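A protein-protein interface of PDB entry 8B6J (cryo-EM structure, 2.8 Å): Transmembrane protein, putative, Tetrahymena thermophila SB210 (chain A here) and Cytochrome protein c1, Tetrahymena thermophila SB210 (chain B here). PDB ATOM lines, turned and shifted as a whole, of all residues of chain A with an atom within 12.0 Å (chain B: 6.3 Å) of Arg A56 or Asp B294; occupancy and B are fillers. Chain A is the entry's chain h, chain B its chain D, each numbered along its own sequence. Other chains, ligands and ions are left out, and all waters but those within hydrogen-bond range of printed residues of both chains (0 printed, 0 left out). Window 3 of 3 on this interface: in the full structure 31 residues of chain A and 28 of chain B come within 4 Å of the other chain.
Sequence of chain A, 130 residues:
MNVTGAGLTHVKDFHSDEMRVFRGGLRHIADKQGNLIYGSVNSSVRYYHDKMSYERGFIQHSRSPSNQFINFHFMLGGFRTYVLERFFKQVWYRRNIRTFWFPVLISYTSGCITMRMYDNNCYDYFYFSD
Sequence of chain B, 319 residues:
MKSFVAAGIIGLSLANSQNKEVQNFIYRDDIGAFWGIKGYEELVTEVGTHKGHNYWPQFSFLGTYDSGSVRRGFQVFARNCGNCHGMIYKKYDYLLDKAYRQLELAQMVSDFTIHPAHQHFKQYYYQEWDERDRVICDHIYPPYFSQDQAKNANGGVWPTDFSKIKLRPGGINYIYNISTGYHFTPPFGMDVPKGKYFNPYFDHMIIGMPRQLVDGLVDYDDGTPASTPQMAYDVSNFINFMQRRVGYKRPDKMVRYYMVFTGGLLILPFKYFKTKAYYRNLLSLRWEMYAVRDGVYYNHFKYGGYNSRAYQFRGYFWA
Arg A56 touches just these residues of chain B: Val B292 and Asp B294. Of the printed residues of chain A, Asp B294 touches Arg A56 (3.1 Å). Of chain A, only Glu A55 (3.9 Å), Gly A57 (3.5 Å) and Phe A58 (3.7 Å) come within 4 Å of Met B289. Val B292 touches just these residues of chain A: Arg A56 and Gly A57. Printed residues of chain B within 4 Å of Glu A55: Met B289 (3.9 Å). Of the printed residues of chain B, Tyr A54 touches Tyr B298. Of the printed residues of chain A, Tyr B290 touches Gly A57 and Ile A59. The nearest residue of chain B that does not touch Arg A56 is Val B296 (4.04 Å). The nearest residue of chain A that does not touch Asp B294 is Gly A57 (8.2 Å).
CB of Tyr B298 touches OH of Tyr A54 (3.5 Å). Met B289 touches Glu A55 (CE to OE2, 3.9 Å). CB of Arg A56 touches CG2 of Val B292, at 3.8 Å. O of Gly A57 touches CA of Met B289, 3.5 Å away. CA of Gly A57 touches CG1 of Val B292, at 3.9 Å. CD1 of Phe A58 touches CG of Met B289, 3.7 Å away. CE1 of Tyr B290 touches CD1 of Ile A59 (3.5 Å).
Of the 10 printed residues of chain B, 5 touch a printed residue of chain A. Printed residues of chain B that touch a printed residue of chain A: Met B289, Tyr B290, Val B292, Asp B294 and Tyr B298. Of the 9 printed residues of chain A, 6 touch a printed residue of chain B. Hydrophobic or aromatic side chains of chain A that line the printed part of chain B: Tyr A54, Phe A58 and Ile A59. Among the printed residues, Asp or Glu carboxylates within 4 Å of a Lys or Arg side-chain nitrogen of the other chain: Arg A56 with Asp B294.
The side-chain carboxylate (OD1) of Asp B294 is in salt-bridge range of the guanidinium group (NH2) of Arg A56, at 3.1 Å. The backbone NH (N) of Tyr B290 sits at hydrogen-bond distance from the backbone carbonyl oxygen (O) of Gly A57, 2.9 Å away.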
ATOM      1  N   MET A  52      29.906  14.026  -5.357  1.00  0.00           N
ATOM      2  CA  MET A  52      29.448  12.789  -4.738  1.00  0.00           C
ATOM      3  C   MET A  52      28.145  12.327  -5.375  1.00  0.00           C
ATOM      4  O   MET A  52      27.189  13.098  -5.496  1.00  0.00           O
ATOM      5  CB  MET A  52      29.257  12.987  -3.234  1.00  0.00           C
ATOM      6  CG  MET A  52      28.642  11.787  -2.524  1.00  0.00           C
ATOM      7  SD  MET A  52      28.656  11.926  -0.725  1.00  0.00           S
ATOM      8  CE  MET A  52      27.605  13.353  -0.476  1.00  0.00           C
ATOM      9  N   SER A  53      28.110  11.059  -5.780  1.00  0.00           N
ATOM     10  CA  SER A  53      26.904  10.480  -6.367  1.00  0.00           C
ATOM     11  C   SER A  53      27.016   8.966  -6.267  1.00  0.00           C
ATOM     12  O   SER A  53      27.902   8.371  -6.890  1.00  0.00           O
ATOM     13  CB  SER A  53      26.735  10.926  -7.813  1.00  0.00           C
ATOM     14  OG  SER A  53      27.812  10.473  -8.614  1.00  0.00           O
ATOM     15  N   TYR A  54      26.125   8.352  -5.495  1.00  0.00           N
ATOM     16  CA  TYR A  54      26.092   6.906  -5.335  1.00  0.00           C
ATOM     17  C   TYR A  54      24.651   6.437  -5.439  1.00  0.00           C
ATOM     18  O   TYR A  54      23.743   7.078  -4.904  1.00  0.00           O
ATOM     19  CB  TYR A  54      26.695   6.481  -3.992  1.00  0.00           C
ATOM     20  CG  TYR A  54      26.818   4.986  -3.819  1.00  0.00           C
ATOM     21  CD1 TYR A  54      27.900   4.296  -4.344  1.00  0.00           C
ATOM     22  CD2 TYR A  54      25.858   4.265  -3.126  1.00  0.00           C
ATOM     23  CE1 TYR A  54      28.020   2.933  -4.187  1.00  0.00           C
ATOM     24  CE2 TYR A  54      25.971   2.901  -2.964  1.00  0.00           C
ATOM     25  CZ  TYR A  54      27.054   2.240  -3.497  1.00  0.00           C
ATOM     26  OH  TYR A  54      27.173   0.880  -3.339  1.00  0.00           O
ATOM     27  N   GLU A  55      24.444   5.315  -6.126  1.00  0.00           N
ATOM     28  CA  GLU A  55      23.100   4.811  -6.355  1.00  0.00           C
ATOM     29  C   GLU A  55      23.160   3.315  -6.617  1.00  0.00           C
ATOM     30  O   GLU A  55      24.111   2.822  -7.227  1.00  0.00           O
ATOM     31  CB  GLU A  55      22.436   5.523  -7.537  1.00  0.00           C
ATOM     32  CG  GLU A  55      21.463   6.622  -7.149  1.00  0.00           C
ATOM     33  CD  GLU A  55      20.142   6.079  -6.649  1.00  0.00           C
ATOM     34  OE1 GLU A  55      20.096   4.897  -6.248  1.00  0.00           O
ATOM     35  OE2 GLU A  55      19.144   6.829  -6.663  1.00  0.00           O
ATOM     36  N   ARG A  56      22.140   2.605  -6.145  1.00  0.00           N
ATOM     37  CA  ARG A  56      21.922   1.207  -6.472  1.00  0.00           C
ATOM     38  C   ARG A  56      20.450   1.016  -6.803  1.00  0.00           C
ATOM     39  O   ARG A  56      19.582   1.678  -6.231  1.00  0.00           O
ATOM     40  CB  ARG A  56      22.309   0.278  -5.316  1.00  0.00           C
ATOM     41  CG  ARG A  56      23.777   0.304  -4.934  1.00  0.00           C
ATOM     42  CD  ARG A  56      24.569  -0.773  -5.650  1.00  0.00           C
ATOM     43  NE  ARG A  56      24.017  -2.106  -5.439  1.00  0.00           N
ATOM     44  CZ  ARG A  56      24.120  -2.792  -4.311  1.00  0.00           C
ATOM     45  NH1 ARG A  56      24.731  -2.292  -3.249  1.00  0.00           N
ATOM     46  NH2 ARG A  56      23.595  -4.012  -4.243  1.00  0.00           N
ATOM     47  N   GLY A  57      20.175   0.108  -7.732  1.00  0.00           N
ATOM     48  CA  GLY A  57      18.793  -0.154  -8.097  1.00  0.00           C
ATOM     49  C   GLY A  57      18.080   1.056  -8.657  1.00  0.00           C
ATOM     50  O   GLY A  57      16.882   1.238  -8.409  1.00  0.00           O
ATOM     51  N   PHE A  58      18.791   1.891  -9.408  1.00  0.00           N
ATOM     52  CA  PHE A  58      18.231   3.095 -10.005  1.00  0.00           C
ATOM     53  C   PHE A  58      18.241   2.953 -11.520  1.00  0.00           C
ATOM     54  O   PHE A  58      19.277   2.632 -12.109  1.00  0.00           O
ATOM     55  CB  PHE A  58      19.023   4.333  -9.582  1.00  0.00           C
ATOM     56  CG  PHE A  58      18.533   5.608 -10.206  1.00  0.00           C
ATOM     57  CD1 PHE A  58      17.483   6.310  -9.643  1.00  0.00           C
ATOM     58  CD2 PHE A  58      19.124   6.103 -11.356  1.00  0.00           C
ATOM     59  CE1 PHE A  58      17.030   7.481 -10.216  1.00  0.00           C
ATOM     60  CE2 PHE A  58      18.674   7.274 -11.931  1.00  0.00           C
ATOM     61  CZ  PHE A  58      17.626   7.963 -11.360  1.00  0.00           C
ATOM     62  N   ILE A  59      17.091   3.191 -12.142  1.00  0.00           N
ATOM     63  CA  ILE A  59      16.941   3.128 -13.590  1.00  0.00           C
ATOM     64  C   ILE A  59      16.289   4.421 -14.050  1.00  0.00           C
ATOM     65  O   ILE A  59      15.300   4.864 -13.456  1.00  0.00           O
ATOM     66  CB  ILE A  59      16.097   1.914 -14.028  1.00  0.00           C
ATOM     67  CG1 ILE A  59      16.692   0.621 -13.470  1.00  0.00           C
ATOM     68  CG2 ILE A  59      16.013   1.843 -15.547  1.00  0.00           C
ATOM     69  CD1 ILE A  59      15.927  -0.622 -13.856  1.00  0.00           C
ATOM     70  N   GLN A  60      16.840   5.029 -15.098  1.00  0.00           N
ATOM     71  CA  GLN A  60      16.233   6.196 -15.714  1.00  0.00           C
ATOM     72  C   GLN A  60      16.077   5.957 -17.208  1.00  0.00           C
ATOM     73  O   GLN A  60      16.882   5.258 -17.829  1.00  0.00           O
ATOM     74  CB  GLN A  60      17.047   7.479 -15.469  1.00  0.00           C
ATOM     75  CG  GLN A  60      18.331   7.611 -16.269  1.00  0.00           C
ATOM     76  CD  GLN A  60      18.844   9.034 -16.289  1.00  0.00           C
ATOM     77  OE1 GLN A  60      19.182   9.569 -17.343  1.00  0.00           O
ATOM     78  NE2 GLN A  60      18.903   9.659 -15.119  1.00  0.00           N
ATOM     79  N   MET B 289      13.207   3.704  -8.827  1.00  0.00           N
ATOM     80  CA  MET B 289      14.059   3.252  -7.736  1.00  0.00           C
ATOM     81  C   MET B 289      13.493   1.961  -7.172  1.00  0.00           C
ATOM     82  O   MET B 289      12.297   1.882  -6.877  1.00  0.00           O
ATOM     83  CB  MET B 289      14.160   4.311  -6.635  1.00  0.00           C
ATOM     84  CG  MET B 289      14.903   5.568  -7.054  1.00  0.00           C
ATOM     85  SD  MET B 289      14.916   6.838  -5.777  1.00  0.00           S
ATOM     86  CE  MET B 289      15.933   6.057  -4.527  1.00  0.00           C
ATOM     87  N   TYR B 290      14.349   0.958  -7.018  1.00  0.00           N
ATOM     88  CA  TYR B 290      13.955  -0.364  -6.551  1.00  0.00           C
ATOM     89  C   TYR B 290      14.641  -0.664  -5.222  1.00  0.00           C
ATOM     90  O   TYR B 290      15.441   0.124  -4.715  1.00  0.00           O
ATOM     91  CB  TYR B 290      14.293  -1.427  -7.597  1.00  0.00           C
ATOM     92  CG  TYR B 290      13.689  -1.146  -8.951  1.00  0.00           C
ATOM     93  CD1 TYR B 290      14.374  -0.398  -9.896  1.00  0.00           C
ATOM     94  CD2 TYR B 290      12.428  -1.620  -9.283  1.00  0.00           C
ATOM     95  CE1 TYR B 290      13.825  -0.135 -11.131  1.00  0.00           C
ATOM     96  CE2 TYR B 290      11.872  -1.362 -10.515  1.00  0.00           C
ATOM     97  CZ  TYR B 290      12.574  -0.619 -11.436  1.00  0.00           C
ATOM     98  OH  TYR B 290      12.026  -0.358 -12.668  1.00  0.00           O
ATOM     99  N   ALA B 291      14.312  -1.822  -4.659  1.00  0.00           N
ATOM    100  CA  ALA B 291      14.819  -2.251  -3.359  1.00  0.00           C
ATOM    101  C   ALA B 291      15.807  -3.391  -3.581  1.00  0.00           C
ATOM    102  O   ALA B 291      15.408  -4.544  -3.755  1.00  0.00           O
ATOM    103  CB  ALA B 291      13.674  -2.678  -2.448  1.00  0.00           C
ATOM    104  N   VAL B 292      17.096  -3.065  -3.563  1.00  0.00           N
ATOM    105  CA  VAL B 292      18.153  -4.063  -3.696  1.00  0.00           C
ATOM    106  C   VAL B 292      18.521  -4.535  -2.294  1.00  0.00           C
ATOM    107  O   VAL B 292      19.094  -3.783  -1.504  1.00  0.00           O
ATOM    108  CB  VAL B 292      19.375  -3.510  -4.440  1.00  0.00           C
ATOM    109  CG1 VAL B 292      19.103  -3.435  -5.927  1.00  0.00           C
ATOM    110  CG2 VAL B 292      19.760  -2.140  -3.919  1.00  0.00           C
ATOM    111  N   ARG B 293      18.178  -5.783  -1.979  1.00  0.00           N
ATOM    112  CA  ARG B 293      18.472  -6.372  -0.680  1.00  0.00           C
ATOM    113  C   ARG B 293      19.315  -7.633  -0.817  1.00  0.00           C
ATOM    114  O   ARG B 293      19.193  -8.561  -0.016  1.00  0.00           O
ATOM    115  CB  ARG B 293      17.183  -6.672   0.083  1.00  0.00           C
ATOM    116  CG  ARG B 293      16.409  -5.434   0.492  1.00  0.00           C
ATOM    117  CD  ARG B 293      15.440  -5.743   1.614  1.00  0.00           C
ATOM    118  NE  ARG B 293      16.136  -6.162   2.824  1.00  0.00           N
ATOM    119  CZ  ARG B 293      15.540  -6.631   3.910  1.00  0.00           C
ATOM    120  NH1 ARG B 293      14.225  -6.761   3.974  1.00  0.00           N
ATOM    121  NH2 ARG B 293      16.280  -6.978   4.958  1.00  0.00           N
ATOM    122  N   ASP B 294      20.172  -7.684  -1.832  1.00  0.00           N
ATOM    123  CA  ASP B 294      21.119  -8.779  -1.948  1.00  0.00           C
ATOM    124  C   ASP B 294      22.232  -8.614  -0.914  1.00  0.00           C
ATOM    125  O   ASP B 294      22.376  -7.570  -0.271  1.00  0.00           O
ATOM    126  CB  ASP B 294      21.695  -8.840  -3.362  1.00  0.00           C
ATOM    127  CG  ASP B 294      22.337  -7.536  -3.788  1.00  0.00           C
ATOM    128  OD1 ASP B 294      21.985  -6.483  -3.218  1.00  0.00           O
ATOM    129  OD2 ASP B 294      23.192  -7.562  -4.697  1.00  0.00           O
ATOM    130  N   GLY B 295      23.031  -9.669  -0.755  1.00  0.00           N
ATOM    131  CA  GLY B 295      24.067  -9.663   0.264  1.00  0.00           C
ATOM    132  C   GLY B 295      25.113  -8.583   0.080  1.00  0.00           C
ATOM    133  O   GLY B 295      25.798  -8.227   1.045  1.00  0.00           O
ATOM    134  N   VAL B 296      25.252  -8.050  -1.134  1.00  0.00           N
ATOM    135  CA  VAL B 296      26.325  -7.104  -1.418  1.00  0.00           C
ATOM    136  C   VAL B 296      26.205  -5.894  -0.505  1.00  0.00           C
ATOM    137  O   VAL B 296      25.119  -5.326  -0.334  1.00  0.00           O
ATOM    138  CB  VAL B 296      26.295  -6.695  -2.897  1.00  0.00           C
ATOM    139  CG1 VAL B 296      27.392  -5.687  -3.193  1.00  0.00           C
ATOM    140  CG2 VAL B 296      26.439  -7.919  -3.787  1.00  0.00           C
ATOM    141  N   TYR B 297      27.327  -5.494   0.085  1.00  0.00           N
ATOM    142  CA  TYR B 297      27.391  -4.314   0.932  1.00  0.00           C
ATOM    143  C   TYR B 297      27.855  -3.112   0.118  1.00  0.00           C
ATOM    144  O   TYR B 297      28.608  -3.246  -0.849  1.00  0.00           O
ATOM    145  CB  TYR B 297      28.338  -4.550   2.109  1.00  0.00           C
ATOM    146  CG  TYR B 297      28.425  -3.395   3.079  1.00  0.00           C
ATOM    147  CD1 TYR B 297      27.447  -3.195   4.041  1.00  0.00           C
ATOM    148  CD2 TYR B 297      29.490  -2.509   3.038  1.00  0.00           C
ATOM    149  CE1 TYR B 297      27.523  -2.144   4.930  1.00  0.00           C
ATOM    150  CE2 TYR B 297      29.576  -1.455   3.924  1.00  0.00           C
ATOM    151  CZ  TYR B 297      28.590  -1.277   4.867  1.00  0.00           C
ATOM    152  OH  TYR B 297      28.672  -0.229   5.751  1.00  0.00           O
ATOM    153  N   TYR B 298      27.399  -1.927   0.524  1.00  0.00           N
ATOM    154  CA  TYR B 298      27.695  -0.691  -0.201  1.00  0.00           C
ATOM    155  C   TYR B 298      29.078  -0.161   0.188  1.00  0.00           C
ATOM    156  O   TYR B 298      29.247   0.960   0.665  1.00  0.00           O
ATOM    157  CB  TYR B 298      26.608   0.347   0.052  1.00  0.00           C
ATOM    158  CG  TYR B 298      26.240   0.540   1.507  1.00  0.00           C
ATOM    159  CD1 TYR B 298      26.927   1.442   2.306  1.00  0.00           C
ATOM    160  CD2 TYR B 298      25.197  -0.175   2.078  1.00  0.00           C
ATOM    161  CE1 TYR B 298      26.592   1.618   3.631  1.00  0.00           C
ATOM    162  CE2 TYR B 298      24.856  -0.005   3.400  1.00  0.00           C
ATOM    163  CZ  TYR B 298      25.555   0.894   4.171  1.00  0.00           C
ATOM    164  OH  TYR B 298      25.215   1.066   5.492  1.00  0.00           O
